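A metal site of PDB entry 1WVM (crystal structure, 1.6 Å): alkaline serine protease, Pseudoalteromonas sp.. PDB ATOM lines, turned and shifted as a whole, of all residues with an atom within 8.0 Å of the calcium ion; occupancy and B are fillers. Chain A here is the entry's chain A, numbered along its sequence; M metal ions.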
ATOM      1  N   ASP A 403      13.102  28.784 -16.277  1.00  0.00           N
ATOM      2  CA  ASP A 403      13.257  29.949 -15.407  1.00  0.00           C
ATOM      3  C   ASP A 403      14.731  30.281 -15.230  1.00  0.00           C
ATOM      4  O   ASP A 403      15.491  29.553 -14.594  1.00  0.00           O
ATOM      5  CB  ASP A 403      12.595  29.679 -14.047  1.00  0.00           C
ATOM      6  CG  ASP A 403      11.108  29.407 -14.170  1.00  0.00           C
ATOM      7  OD1 ASP A 403      10.406  30.209 -14.828  1.00  0.00           O
ATOM      8  OD2 ASP A 403      10.637  28.390 -13.609  1.00  0.00           O
ATOM      9  N   ASP A 404      15.132  31.416 -15.795  1.00  0.00           N
ATOM     10  CA  ASP A 404      16.519  31.889 -15.739  1.00  0.00           C
ATOM     11  C   ASP A 404      17.081  31.866 -14.320  1.00  0.00           C
ATOM     12  O   ASP A 404      16.489  32.415 -13.389  1.00  0.00           O
ATOM     13  CB  ASP A 404      16.592  33.306 -16.314  1.00  0.00           C
ATOM     14  CG  ASP A 404      18.010  33.764 -16.548  1.00  0.00           C
ATOM     15  OD1 ASP A 404      18.947  32.950 -16.410  1.00  0.00           O
ATOM     16  OD2 ASP A 404      18.190  34.964 -16.884  1.00  0.00           O
ATOM     17  N   LEU A 405      18.235  31.209 -14.147  1.00  0.00           N
ATOM     18  CA  LEU A 405      18.884  31.122 -12.846  1.00  0.00           C
ATOM     19  C   LEU A 405      20.249  31.792 -12.884  1.00  0.00           C
ATOM     20  O   LEU A 405      20.718  32.215 -13.943  1.00  0.00           O
ATOM     21  CB  LEU A 405      19.069  29.659 -12.438  1.00  0.00           C
ATOM     22  CG  LEU A 405      17.841  28.745 -12.362  1.00  0.00           C
ATOM     23  CD1 LEU A 405      18.286  27.372 -11.893  1.00  0.00           C
ATOM     24  CD2 LEU A 405      16.811  29.330 -11.417  1.00  0.00           C
ATOM     25  N   SER A 406      20.887  31.888 -11.723  1.00  0.00           N
ATOM     26  CA  SER A 406      22.212  32.492 -11.613  1.00  0.00           C
ATOM     27  C   SER A 406      22.237  33.851 -12.313  1.00  0.00           C
ATOM     28  O   SER A 406      21.264  34.599 -12.265  1.00  0.00           O
ATOM     29  CB  SER A 406      23.256  31.554 -12.244  1.00  0.00           C
ATOM     30  OG  SER A 406      24.574  32.018 -12.010  1.00  0.00           O
ATOM     31  N   VAL A 407      23.354  34.167 -12.973  1.00  0.00           N
ATOM     32  CA  VAL A 407      23.486  35.430 -13.679  1.00  0.00           C
ATOM     33  C   VAL A 407      22.472  35.494 -14.825  1.00  0.00           C
ATOM     34  O   VAL A 407      22.076  34.460 -15.371  1.00  0.00           O
ATOM     35  CB  VAL A 407      24.919  35.615 -14.225  1.00  0.00           C
ATOM     36  CG1 VAL A 407      25.216  34.554 -15.268  1.00  0.00           C
ATOM     37  CG2 VAL A 407      25.080  37.013 -14.801  1.00  0.00           C
ATOM     38  N   ALA A 408      22.060  36.703 -15.189  1.00  0.00           N
ATOM     39  CA  ALA A 408      21.089  36.886 -16.264  1.00  0.00           C
ATOM     40  C   ALA A 408      21.524  36.207 -17.565  1.00  0.00           C
ATOM     41  O   ALA A 408      22.691  36.247 -17.931  1.00  0.00           O
ATOM     42  CB  ALA A 408      20.870  38.374 -16.508  1.00  0.00           C
ATOM     43  N   GLY A 409      20.569  35.583 -18.239  1.00  0.00           N
ATOM     44  CA  GLY A 409      20.849  34.903 -19.491  1.00  0.00           C
ATOM     45  C   GLY A 409      21.440  33.523 -19.320  1.00  0.00           C
ATOM     46  O   GLY A 409      21.744  33.103 -18.212  1.00  0.00           O
ATOM     47  N   ARG A 410      21.612  32.811 -20.435  1.00  0.00           N
ATOM     48  CA  ARG A 410      22.181  31.474 -20.392  1.00  0.00           C
ATOM     49  C   ARG A 410      23.602  31.522 -19.852  1.00  0.00           C
ATOM     50  O   ARG A 410      24.390  32.394 -20.223  1.00  0.00           O
ATOM     51  CB  ARG A 410      22.201  30.862 -21.803  1.00  0.00           C
ATOM     52  CG  ARG A 410      22.763  29.452 -21.859  1.00  0.00           C
ATOM     53  CD  ARG A 410      22.766  28.911 -23.270  1.00  0.00           C
ATOM     54  NE  ARG A 410      23.199  27.512 -23.318  1.00  0.00           N
ATOM     55  CZ  ARG A 410      23.158  26.748 -24.396  1.00  0.00           C
ATOM     56  NH1 ARG A 410      23.569  25.493 -24.332  1.00  0.00           N
ATOM     57  NH2 ARG A 410      22.700  27.230 -25.545  1.00  0.00           N
ATOM     58  N   ASP A 411      23.917  30.599 -18.947  1.00  0.00           N
ATOM     59  CA  ASP A 411      25.250  30.511 -18.368  1.00  0.00           C
ATOM     60  C   ASP A 411      25.682  29.046 -18.376  1.00  0.00           C
ATOM     61  O   ASP A 411      24.845  28.156 -18.553  1.00  0.00           O
ATOM     62  CB  ASP A 411      25.280  31.078 -16.939  1.00  0.00           C
ATOM     63  CG  ASP A 411      24.199  30.505 -16.055  1.00  0.00           C
ATOM     64  OD1 ASP A 411      23.150  31.154 -15.906  1.00  0.00           O
ATOM     65  OD2 ASP A 411      24.409  29.400 -15.508  1.00  0.00           O
ATOM     66  N   ASN A 412      26.974  28.802 -18.196  1.00  0.00           N
ATOM     67  CA  ASN A 412      27.500  27.441 -18.231  1.00  0.00           C
ATOM     68  C   ASN A 412      27.124  26.586 -17.033  1.00  0.00           C
ATOM     69  O   ASN A 412      27.206  25.353 -17.099  1.00  0.00           O
ATOM     70  CB  ASN A 412      29.026  27.471 -18.361  1.00  0.00           C
ATOM     71  CG  ASN A 412      29.505  28.008 -19.706  1.00  0.00           C
ATOM     72  OD1 ASN A 412      30.693  27.961 -20.010  1.00  0.00           O
ATOM     73  ND2 ASN A 412      28.574  28.520 -20.504  1.00  0.00           N
ATOM     74  N   GLN A 413      26.715  27.214 -15.938  1.00  0.00           N
ATOM     75  CA  GLN A 413      26.344  26.464 -14.741  1.00  0.00           C
ATOM     76  C   GLN A 413      24.918  25.927 -14.781  1.00  0.00           C
ATOM     77  O   GLN A 413      24.683  24.770 -14.427  1.00  0.00           O
ATOM     78  CB  GLN A 413      26.508  27.326 -13.486  1.00  0.00           C
ATOM     79  CG  GLN A 413      27.956  27.489 -13.024  1.00  0.00           C
ATOM     80  CD  GLN A 413      28.744  28.444 -13.898  1.00  0.00           C
ATOM     81  OE1 GLN A 413      29.977  28.351 -13.966  1.00  0.00           O
ATOM     82  NE2 GLN A 413      28.062  29.371 -14.542  1.00  0.00           N
ATOM     83  N   THR A 414      23.972  26.761 -15.209  1.00  0.00           N
ATOM     84  CA  THR A 414      22.569  26.367 -15.223  1.00  0.00           C
ATOM     85  C   THR A 414      21.860  26.399 -16.586  1.00  0.00           C
ATOM     86  O   THR A 414      20.662  26.152 -16.669  1.00  0.00           O
ATOM     87  CB  THR A 414      21.753  27.252 -14.252  1.00  0.00           C
ATOM     88  OG1 THR A 414      21.805  28.618 -14.692  1.00  0.00           O
ATOM     89  CG2 THR A 414      22.335  27.163 -12.855  1.00  0.00           C
ATOM     90  N   GLY A 415      22.613  26.683 -17.645  1.00  0.00           N
ATOM     91  CA  GLY A 415      21.998  26.730 -18.962  1.00  0.00           C
ATOM     92  C   GLY A 415      20.937  27.815 -19.009  1.00  0.00           C
ATOM     93  O   GLY A 415      21.145  28.920 -18.498  1.00  0.00           O
ATOM     94  N   TYR A 416      19.796  27.514 -19.604  1.00  0.00           N
ATOM     95  CA  TYR A 416      18.709  28.481 -19.695  1.00  0.00           C
ATOM     96  C   TYR A 416      17.954  28.625 -18.376  1.00  0.00           C
ATOM     97  O   TYR A 416      17.126  29.519 -18.227  1.00  0.00           O
ATOM     98  CB  TYR A 416      17.747  28.098 -20.811  1.00  0.00           C
ATOM     99  CG  TYR A 416      18.331  28.318 -22.194  1.00  0.00           C
ATOM    100  CD1 TYR A 416      18.634  29.602 -22.642  1.00  0.00           C
ATOM    101  CD2 TYR A 416      18.597  27.247 -23.036  1.00  0.00           C
ATOM    102  CE1 TYR A 416      19.197  29.815 -23.897  1.00  0.00           C
ATOM    103  CE2 TYR A 416      19.154  27.449 -24.298  1.00  0.00           C
ATOM    104  CZ  TYR A 416      19.451  28.737 -24.719  1.00  0.00           C
ATOM    105  OH  TYR A 416      20.015  28.938 -25.957  1.00  0.00           O
ATOM    106  N   GLY A 417      18.242  27.736 -17.423  1.00  0.00           N
ATOM    107  CA  GLY A 417      17.582  27.812 -16.139  1.00  0.00           C
ATOM    108  C   GLY A 417      16.830  26.557 -15.729  1.00  0.00           C
ATOM    109  O   GLY A 417      17.020  25.476 -16.286  1.00  0.00           O
ATOM    110  N   MET A 418      15.947  26.724 -14.746  1.00  0.00           N
ATOM    111  CA  MET A 418      15.148  25.629 -14.226  1.00  0.00           C
ATOM    112  C   MET A 418      13.998  25.251 -15.154  1.00  0.00           C
ATOM    113  O   MET A 418      13.218  26.117 -15.561  1.00  0.00           O
ATOM    114  CB  MET A 418      14.590  25.995 -12.850  1.00  0.00           C
ATOM    115  CG  MET A 418      13.881  24.848 -12.171  1.00  0.00           C
ATOM    116  SD  MET A 418      15.036  23.543 -11.742  1.00  0.00           S
ATOM    117  CE  MET A 418      14.422  23.065 -10.112  1.00  0.00           C
HETATM  118 CA    CA M   1      21.185  32.401 -16.141  1.00  0.00          CA
HETATM  119 MG    MG M   2      20.331  30.202 -16.180  1.00  0.00          MG
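OD2 of Asp 411 is in hydrogen-bond range of N of Thr 414 (2.7 Å). N of Gln 413 is in hydrogen-bond range of OD2 of Asp 411 (3.2 Å).
Along chain A the residues within 4 Å of the calcium ion span positions 404 to 411. The nearest printed residue that does not touch the calcium ion is Ala 408 (4.1 Å).
The calcium ion is bound by O of Leu 405, at 2.3 Å. The calcium ion is bound by the backbone carbonyl oxygen (O) of Gly 409 (2.3 Å). The side-chain carboxylate (OD1) of Asp 404 binds the calcium ion (2.3 Å). OD1 of Asp 411 is bound to the calcium ion. O of Val 407 binds the calcium ion.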
